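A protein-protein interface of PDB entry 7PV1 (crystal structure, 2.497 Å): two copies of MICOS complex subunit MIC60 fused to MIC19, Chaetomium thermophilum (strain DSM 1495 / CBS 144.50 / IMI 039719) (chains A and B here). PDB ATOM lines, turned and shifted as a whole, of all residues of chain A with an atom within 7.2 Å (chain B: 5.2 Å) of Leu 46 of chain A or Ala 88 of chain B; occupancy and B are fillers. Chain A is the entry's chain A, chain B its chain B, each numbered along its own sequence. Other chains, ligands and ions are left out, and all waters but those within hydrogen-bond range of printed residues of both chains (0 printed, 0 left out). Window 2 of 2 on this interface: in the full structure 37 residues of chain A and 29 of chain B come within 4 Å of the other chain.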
ATOM      1  N   THR A   3     -11.398  -0.028  18.869  1.00  0.00           N
ATOM      2  CA  THR A   3     -11.836   0.325  17.525  1.00  0.00           C
ATOM      3  C   THR A   3     -10.681   0.230  16.533  1.00  0.00           C
ATOM      4  O   THR A   3     -10.889   0.268  15.320  1.00  0.00           O
ATOM      5  CB  THR A   3     -12.434   1.746  17.480  1.00  0.00           C
ATOM      6  OG1 THR A   3     -13.547   1.826  18.379  1.00  0.00           O
ATOM      7  CG2 THR A   3     -12.905   2.086  16.073  1.00  0.00           C
ATOM      8  N   ARG A   4      -9.457   0.108  17.053  1.00  0.00           N
ATOM      9  CA  ARG A   4      -8.308  -0.061  16.171  1.00  0.00           C
ATOM     10  C   ARG A   4      -8.402  -1.364  15.391  1.00  0.00           C
ATOM     11  O   ARG A   4      -7.966  -1.430  14.235  1.00  0.00           O
ATOM     12  CB  ARG A   4      -7.009  -0.008  16.979  1.00  0.00           C
ATOM     13  CG  ARG A   4      -5.744  -0.211  16.154  1.00  0.00           C
ATOM     14  CD  ARG A   4      -4.492  -0.008  16.997  1.00  0.00           C
ATOM     15  NE  ARG A   4      -4.390   1.346  17.540  1.00  0.00           N
ATOM     16  CZ  ARG A   4      -3.491   1.715  18.447  1.00  0.00           C
ATOM     17  NH1 ARG A   4      -2.620   0.830  18.913  1.00  0.00           N
ATOM     18  NH2 ARG A   4      -3.462   2.966  18.891  1.00  0.00           N
ATOM     19  N   LEU A   7     -10.842  -0.715  12.777  1.00  0.00           N
ATOM     20  CA  LEU A   7     -10.226   0.188  11.813  1.00  0.00           C
ATOM     21  C   LEU A   7      -9.428  -0.593  10.772  1.00  0.00           C
ATOM     22  O   LEU A   7      -9.438  -0.251   9.584  1.00  0.00           O
ATOM     23  CB  LEU A   7      -9.341   1.196  12.552  1.00  0.00           C
ATOM     24  CG  LEU A   7      -8.986   2.539  11.905  1.00  0.00           C
ATOM     25  CD1 LEU A   7     -10.242   3.284  11.479  1.00  0.00           C
ATOM     26  CD2 LEU A   7      -8.150   3.389  12.852  1.00  0.00           C
ATOM     27  N   ILE A   8      -8.735  -1.649  11.205  1.00  0.00           N
ATOM     28  CA  ILE A   8      -7.928  -2.453  10.290  1.00  0.00           C
ATOM     29  C   ILE A   8      -8.809  -3.154   9.267  1.00  0.00           C
ATOM     30  O   ILE A   8      -8.464  -3.242   8.082  1.00  0.00           O
ATOM     31  CB  ILE A   8      -7.095  -3.473  11.085  1.00  0.00           C
ATOM     32  CG1 ILE A   8      -6.171  -2.751  12.064  1.00  0.00           C
ATOM     33  CG2 ILE A   8      -6.320  -4.381  10.129  1.00  0.00           C
ATOM     34  CD1 ILE A   8      -5.579  -3.651  13.131  1.00  0.00           C
ATOM     35  N   PHE A  40       0.957  -0.432   9.105  1.00  0.00           N
ATOM     36  CA  PHE A  40       0.906   0.512  10.217  1.00  0.00           C
ATOM     37  C   PHE A  40      -0.276   0.227  11.132  1.00  0.00           C
ATOM     38  O   PHE A  40      -0.170   0.370  12.355  1.00  0.00           O
ATOM     39  CB  PHE A  40       0.829   1.945   9.693  1.00  0.00           C
ATOM     40  CG  PHE A  40       2.159   2.523   9.296  1.00  0.00           C
ATOM     41  CD1 PHE A  40       3.256   2.406  10.133  1.00  0.00           C
ATOM     42  CD2 PHE A  40       2.308   3.195   8.094  1.00  0.00           C
ATOM     43  CE1 PHE A  40       4.477   2.941   9.775  1.00  0.00           C
ATOM     44  CE2 PHE A  40       3.528   3.731   7.731  1.00  0.00           C
ATOM     45  CZ  PHE A  40       4.614   3.604   8.572  1.00  0.00           C
ATOM     46  N   LEU A  41      -1.414  -0.165  10.558  1.00  0.00           N
ATOM     47  CA  LEU A  41      -2.592  -0.444  11.370  1.00  0.00           C
ATOM     48  C   LEU A  41      -2.371  -1.657  12.267  1.00  0.00           C
ATOM     49  O   LEU A  41      -2.765  -1.650  13.439  1.00  0.00           O
ATOM     50  CB  LEU A  41      -3.806  -0.647  10.465  1.00  0.00           C
ATOM     51  CG  LEU A  41      -4.242   0.645   9.769  1.00  0.00           C
ATOM     52  CD1 LEU A  41      -5.287   0.375   8.695  1.00  0.00           C
ATOM     53  CD2 LEU A  41      -4.735   1.665  10.789  1.00  0.00           C
ATOM     54  N   GLU A  42      -1.746  -2.711  11.735  1.00  0.00           N
ATOM     55  CA  GLU A  42      -1.500  -3.904  12.541  1.00  0.00           C
ATOM     56  C   GLU A  42      -0.576  -3.601  13.713  1.00  0.00           C
ATOM     57  O   GLU A  42      -0.771  -4.124  14.816  1.00  0.00           O
ATOM     58  CB  GLU A  42      -0.901  -5.010  11.673  1.00  0.00           C
ATOM     59  CG  GLU A  42      -1.848  -5.622  10.648  1.00  0.00           C
ATOM     60  CD  GLU A  42      -2.780  -6.656  11.255  1.00  0.00           C
ATOM     61  OE1 GLU A  42      -2.652  -6.941  12.464  1.00  0.00           O
ATOM     62  OE2 GLU A  42      -3.629  -7.199  10.519  1.00  0.00           O
ATOM     63  N   GLU A  43       0.440  -2.765  13.496  1.00  0.00           N
ATOM     64  CA  GLU A  43       1.347  -2.391  14.574  1.00  0.00           C
ATOM     65  C   GLU A  43       0.769  -1.323  15.494  1.00  0.00           C
ATOM     66  O   GLU A  43       1.402  -0.984  16.499  1.00  0.00           O
ATOM     67  CB  GLU A  43       2.685  -1.923  13.991  1.00  0.00           C
ATOM     68  CG  GLU A  43       3.049  -0.486  14.311  1.00  0.00           C
ATOM     69  CD  GLU A  43       4.303  -0.030  13.590  1.00  0.00           C
ATOM     70  OE1 GLU A  43       5.164  -0.886  13.282  1.00  0.00           O
ATOM     71  OE2 GLU A  43       4.427   1.181  13.320  1.00  0.00           O
ATOM     72  N   GLY A  44      -0.411  -0.787  15.184  1.00  0.00           N
ATOM     73  CA  GLY A  44      -1.029   0.212  16.032  1.00  0.00           C
ATOM     74  C   GLY A  44      -0.504   1.620  15.868  1.00  0.00           C
ATOM     75  O   GLY A  44      -0.784   2.470  16.722  1.00  0.00           O
ATOM     76  N   ASP A  45       0.248   1.896  14.804  1.00  0.00           N
ATOM     77  CA  ASP A  45       0.813   3.225  14.570  1.00  0.00           C
ATOM     78  C   ASP A  45      -0.172   4.049  13.739  1.00  0.00           C
ATOM     79  O   ASP A  45       0.035   4.345  12.561  1.00  0.00           O
ATOM     80  CB  ASP A  45       2.171   3.105  13.890  1.00  0.00           C
ATOM     81  CG  ASP A  45       2.948   4.405  13.895  1.00  0.00           C
ATOM     82  OD1 ASP A  45       2.349   5.460  14.183  1.00  0.00           O
ATOM     83  OD2 ASP A  45       4.165   4.369  13.607  1.00  0.00           O
ATOM     84  N   LEU A  46      -1.272   4.425  14.400  1.00  0.00           N
ATOM     85  CA  LEU A  46      -2.342   5.148  13.720  1.00  0.00           C
ATOM     86  C   LEU A  46      -1.851   6.458  13.118  1.00  0.00           C
ATOM     87  O   LEU A  46      -2.228   6.809  11.994  1.00  0.00           O
ATOM     88  CB  LEU A  46      -3.497   5.405  14.689  1.00  0.00           C
ATOM     89  CG  LEU A  46      -4.100   4.166  15.356  1.00  0.00           C
ATOM     90  CD1 LEU A  46      -5.280   4.548  16.234  1.00  0.00           C
ATOM     91  CD2 LEU A  46      -4.521   3.146  14.309  1.00  0.00           C
ATOM     92  N   ASP A  47      -1.012   7.198  13.844  1.00  0.00           N
ATOM     93  CA  ASP A  47      -0.531   8.474  13.326  1.00  0.00           C
ATOM     94  C   ASP A  47       0.186   8.278  11.996  1.00  0.00           C
ATOM     95  O   ASP A  47      -0.081   8.988  11.020  1.00  0.00           O
ATOM     96  CB  ASP A  47       0.377   9.160  14.348  1.00  0.00           C
ATOM     97  CG  ASP A  47       0.617  10.626  14.023  1.00  0.00           C
ATOM     98  OD1 ASP A  47       1.165  10.920  12.939  1.00  0.00           O
ATOM     99  OD2 ASP A  47       0.237  11.488  14.845  1.00  0.00           O
ATOM    100  N   ASN A  48       1.107   7.312  11.941  1.00  0.00           N
ATOM    101  CA  ASN A  48       1.812   7.033  10.695  1.00  0.00           C
ATOM    102  C   ASN A  48       0.867   6.480   9.634  1.00  0.00           C
ATOM    103  O   ASN A  48       1.017   6.781   8.444  1.00  0.00           O
ATOM    104  CB  ASN A  48       2.957   6.053  10.946  1.00  0.00           C
ATOM    105  CG  ASN A  48       4.240   6.747  11.351  1.00  0.00           C
ATOM    106  OD1 ASN A  48       4.569   7.817  10.837  1.00  0.00           O
ATOM    107  ND2 ASN A  48       4.974   6.141  12.277  1.00  0.00           N
ATOM    108  N   ALA A  49      -0.113   5.670  10.045  1.00  0.00           N
ATOM    109  CA  ALA A  49      -1.075   5.130   9.089  1.00  0.00           C
ATOM    110  C   ALA A  49      -1.848   6.243   8.393  1.00  0.00           C
ATOM    111  O   ALA A  49      -2.026   6.218   7.171  1.00  0.00           O
ATOM    112  CB  ALA A  49      -2.034   4.172   9.797  1.00  0.00           C
ATOM    113  N   ALA A  50      -2.326   7.228   9.159  1.00  0.00           N
ATOM    114  CA  ALA A  50      -3.017   8.360   8.551  1.00  0.00           C
ATOM    115  C   ALA A  50      -2.081   9.165   7.662  1.00  0.00           C
ATOM    116  O   ALA A  50      -2.515   9.732   6.652  1.00  0.00           O
ATOM    117  CB  ALA A  50      -3.624   9.253   9.633  1.00  0.00           C
ATOM    118  N   ARG A  51      -0.801   9.232   8.029  1.00  0.00           N
ATOM    119  CA  ARG A  51       0.180   9.935   7.210  1.00  0.00           C
ATOM    120  C   ARG A  51       0.312   9.284   5.839  1.00  0.00           C
ATOM    121  O   ARG A  51       0.307   9.968   4.810  1.00  0.00           O
ATOM    122  CB  ARG A  51       1.523   9.956   7.935  1.00  0.00           C
ATOM    123  CG  ARG A  51       2.622  10.689   7.206  1.00  0.00           C
ATOM    124  CD  ARG A  51       3.973  10.169   7.653  1.00  0.00           C
ATOM    125  NE  ARG A  51       4.201   8.810   7.171  1.00  0.00           N
ATOM    126  CZ  ARG A  51       5.086   7.973   7.697  1.00  0.00           C
ATOM    127  NH1 ARG A  51       5.820   8.352   8.732  1.00  0.00           N
ATOM    128  NH2 ARG A  51       5.232   6.755   7.192  1.00  0.00           N
ATOM    129  N   GLU A  52       0.440   7.955   5.812  1.00  0.00           N
ATOM    130  CA  GLU A  52       0.489   7.232   4.545  1.00  0.00           C
ATOM    131  C   GLU A  52      -0.788   7.436   3.739  1.00  0.00           C
ATOM    132  O   GLU A  52      -0.734   7.633   2.519  1.00  0.00           O
ATOM    133  CB  GLU A  52       0.724   5.742   4.802  1.00  0.00           C
ATOM    134  CG  GLU A  52       2.145   5.370   5.199  1.00  0.00           C
ATOM    135  CD  GLU A  52       3.077   5.261   4.007  1.00  0.00           C
ATOM    136  OE1 GLU A  52       3.898   6.180   3.801  1.00  0.00           O
ATOM    137  OE2 GLU A  52       2.982   4.257   3.272  1.00  0.00           O
ATOM    138  N   MET A  53      -1.948   7.394   4.403  1.00  0.00           N
ATOM    139  CA  MET A  53      -3.221   7.522   3.698  1.00  0.00           C
ATOM    140  C   MET A  53      -3.359   8.855   2.974  1.00  0.00           C
ATOM    141  O   MET A  53      -4.097   8.949   1.986  1.00  0.00           O
ATOM    142  CB  MET A  53      -4.380   7.379   4.686  1.00  0.00           C
ATOM    143  CG  MET A  53      -4.804   5.972   5.037  1.00  0.00           C
ATOM    144  SD  MET A  53      -6.139   6.060   6.246  1.00  0.00           S
ATOM    145  CE  MET A  53      -7.168   4.694   5.727  1.00  0.00           C
ATOM    146  N   VAL B  83     -12.702   9.097   5.522  1.00  0.00           N
ATOM    147  CA  VAL B  83     -13.389   8.756   6.763  1.00  0.00           C
ATOM    148  C   VAL B  83     -12.481   7.907   7.643  1.00  0.00           C
ATOM    149  O   VAL B  83     -12.376   8.132   8.855  1.00  0.00           O
ATOM    150  CB  VAL B  83     -14.724   8.050   6.463  1.00  0.00           C
ATOM    151  CG1 VAL B  83     -15.390   7.590   7.752  1.00  0.00           C
ATOM    152  CG2 VAL B  83     -15.641   8.981   5.689  1.00  0.00           C
ATOM    153  N   ILE B  84     -11.794   6.933   7.045  1.00  0.00           N
ATOM    154  CA  ILE B  84     -10.852   6.121   7.809  1.00  0.00           C
ATOM    155  C   ILE B  84      -9.682   6.976   8.286  1.00  0.00           C
ATOM    156  O   ILE B  84      -9.228   6.846   9.427  1.00  0.00           O
ATOM    157  CB  ILE B  84     -10.373   4.921   6.971  1.00  0.00           C
ATOM    158  CG1 ILE B  84     -11.565   4.070   6.529  1.00  0.00           C
ATOM    159  CG2 ILE B  84      -9.412   4.068   7.776  1.00  0.00           C
ATOM    160  CD1 ILE B  84     -11.180   2.803   5.785  1.00  0.00           C
ATOM    161  N   GLN B  85      -9.176   7.863   7.423  1.00  0.00           N
ATOM    162  CA  GLN B  85      -8.059   8.720   7.809  1.00  0.00           C
ATOM    163  C   GLN B  85      -8.431   9.629   8.972  1.00  0.00           C
ATOM    164  O   GLN B  85      -7.689   9.739   9.954  1.00  0.00           O
ATOM    165  CB  GLN B  85      -7.598   9.561   6.618  1.00  0.00           C
ATOM    166  CG  GLN B  85      -6.433  10.479   6.952  1.00  0.00           C
ATOM    167  CD  GLN B  85      -5.950  11.274   5.760  1.00  0.00           C
ATOM    168  OE1 GLN B  85      -6.054  10.830   4.616  1.00  0.00           O
ATOM    169  NE2 GLN B  85      -5.430  12.468   6.021  1.00  0.00           N
ATOM    170  N   ALA B  86      -9.593  10.280   8.886  1.00  0.00           N
ATOM    171  CA  ALA B  86     -10.024  11.147   9.976  1.00  0.00           C
ATOM    172  C   ALA B  86     -10.298  10.338  11.234  1.00  0.00           C
ATOM    173  O   ALA B  86     -10.013  10.794  12.348  1.00  0.00           O
ATOM    174  CB  ALA B  86     -11.267  11.934   9.561  1.00  0.00           C
ATOM    175  N   GLU B  87     -10.845   9.134  11.074  1.00  0.00           N
ATOM    176  CA  GLU B  87     -11.086   8.281  12.228  1.00  0.00           C
ATOM    177  C   GLU B  87      -9.767   7.859  12.867  1.00  0.00           C
ATOM    178  O   GLU B  87      -9.656   7.797  14.097  1.00  0.00           O
ATOM    179  CB  GLU B  87     -11.909   7.065  11.805  1.00  0.00           C
ATOM    180  CG  GLU B  87     -12.480   6.272  12.955  1.00  0.00           C
ATOM    181  CD  GLU B  87     -13.653   6.981  13.607  1.00  0.00           C
ATOM    182  OE1 GLU B  87     -14.606   7.349  12.887  1.00  0.00           O
ATOM    183  OE2 GLU B  87     -13.611   7.189  14.837  1.00  0.00           O
ATOM    184  N   ALA B  88      -8.752   7.581  12.044  1.00  0.00           N
ATOM    185  CA  ALA B  88      -7.444   7.204  12.572  1.00  0.00           C
ATOM    186  C   ALA B  88      -6.818   8.349  13.359  1.00  0.00           C
ATOM    187  O   ALA B  88      -6.363   8.161  14.494  1.00  0.00           O
ATOM    188  CB  ALA B  88      -6.526   6.766  11.430  1.00  0.00           C
ATOM    189  N   ARG B  89      -6.779   9.546  12.768  1.00  0.00           N
ATOM    190  CA  ARG B  89      -6.260  10.706  13.486  1.00  0.00           C
ATOM    191  C   ARG B  89      -6.972  10.891  14.821  1.00  0.00           C
ATOM    192  O   ARG B  89      -6.348  11.265  15.822  1.00  0.00           O
ATOM    193  CB  ARG B  89      -6.391  11.968  12.626  1.00  0.00           C
ATOM    194  CG  ARG B  89      -5.329  12.105  11.544  1.00  0.00           C
ATOM    195  CD  ARG B  89      -5.472  13.403  10.752  1.00  0.00           C
ATOM    196  NE  ARG B  89      -6.345  13.258   9.588  1.00  0.00           N
ATOM    197  CZ  ARG B  89      -7.501  13.895   9.429  1.00  0.00           C
ATOM    198  NH1 ARG B  89      -7.934  14.738  10.359  1.00  0.00           N
ATOM    199  NH2 ARG B  89      -8.223  13.695   8.333  1.00  0.00           N
ATOM    200  N   LEU B  90      -8.278  10.620  14.858  1.00  0.00           N
ATOM    201  CA  LEU B  90      -9.038  10.802  16.089  1.00  0.00           C
ATOM    202  C   LEU B  90      -8.556   9.854  17.181  1.00  0.00           C
ATOM    203  O   LEU B  90      -8.352  10.266  18.326  1.00  0.00           O
ATOM    204  CB  LEU B  90     -10.530  10.608  15.820  1.00  0.00           C
ATOM    205  CG  LEU B  90     -11.448  10.743  17.034  1.00  0.00           C
ATOM    206  CD1 LEU B  90     -11.147  12.028  17.789  1.00  0.00           C
ATOM    207  CD2 LEU B  90     -12.910  10.699  16.612  1.00  0.00           C
ATOM    208  N   GLN B  91      -8.360   8.576  16.842  1.00  0.00           N
ATOM    209  CA  GLN B  91      -7.900   7.623  17.848  1.00  0.00           C
ATOM    210  C   GLN B  91      -6.467   7.887  18.286  1.00  0.00           C
ATOM    211  O   GLN B  91      -6.101   7.551  19.418  1.00  0.00           O
ATOM    212  CB  GLN B  91      -8.009   6.194  17.321  1.00  0.00           C
ATOM    213  CG  GLN B  91      -9.424   5.632  17.269  1.00  0.00           C
ATOM    214  CD  GLN B  91      -9.424   4.135  17.010  1.00  0.00           C
ATOM    215  OE1 GLN B  91     -10.299   3.611  16.317  1.00  0.00           O
ATOM    216  NE2 GLN B  91      -8.442   3.440  17.569  1.00  0.00           N
ATOM    217  N   SER B  92      -5.640   8.480  17.418  1.00  0.00           N
ATOM    218  CA  SER B  92      -4.269   8.790  17.816  1.00  0.00           C
ATOM    219  C   SER B  92      -4.247   9.772  18.980  1.00  0.00           C
ATOM    220  O   SER B  92      -3.353   9.710  19.832  1.00  0.00           O
ATOM    221  CB  SER B  92      -3.470   9.339  16.632  1.00  0.00           C
ATOM    222  OG  SER B  92      -3.743  10.713  16.417  1.00  0.00           O
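Glu 42 of chain A touches none of the printed residues of chain B. Gly 44 of chain A touches none of the printed residues of chain B. Of the printed residues of chain B, Leu 46 of chain A touches Ala 88 and Gln 91. Of the printed residues of chain B, Met 53 of chain A touches Ile 84 (3.1 Å) and Gln 85 (3.6 Å). Of the printed residues of chain A, Gln 85 of chain B touches Ala 50 and Met 53. Of the printed residues of chain A, Ala 88 of chain B touches Leu 7 (3.9 Å) and Leu 46 (3.98 Å). The nearest printed residue of chain B that does not touch Arg 4 of chain A is Ser 92 of chain B (6.0 Å).
Hydrophobic or aromatic side chains of chain A within 4 Å of the printed part of chain B: Leu 7, Leu 46, Ala 50 and Met 53. Printed residues of chain B that touch a printed residue of chain A: Ile 84, Gln 85, Ala 88, Arg 89 and Gln 91. Hydrophobic or aromatic side chains of chain B within 4 Å of the printed part of chain A: Ile 84. Along chain B the printed residues that touch a printed residue of chain A span positions 84 to 91. Among the printed residues, 10 pairs touch across the chains. Among the printed residues, no Asp or Glu carboxylate lies within 4 Å of a Lys or Arg side-chain nitrogen of the other chain.
Among the printed residues, merely in contact across the chains: Thr 3 of chain A with Gln 91 of chain B, Arg 4 of chain A with Gln 91 of chain B, Leu 7 of chain A with Ile 84 of chain B, Leu 7 of chain A with Ala 88 of chain B, Leu 46 of chain A with Ala 88 of chain B, Leu 46 of chain A with Gln 91 of chain B, Ala 50 of chain A with Gln 85 of chain B, Ala 50 of chain A with Arg 89 of chain B and Met 53 of chain A with Ile 84 of chain B.
The guanidinium group (NH1) of Arg 4 of chain A sits at hydrogen-bond distance from the backbone carbonyl oxygen (O) of Gly 44 of chain A, at 3.3 Å. OG of Ser 92 of chain B lies within hydrogen-bond range of O of Arg 89 of chain B, 2.7 Å away.
N of Gln 85 of chain B lies close to SD of Met 53 of chain A.
No position is printed for both chains. Of the 10 pairs that touch across the chains among the printed residues, none has its exchanged pair printed and touching as well.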
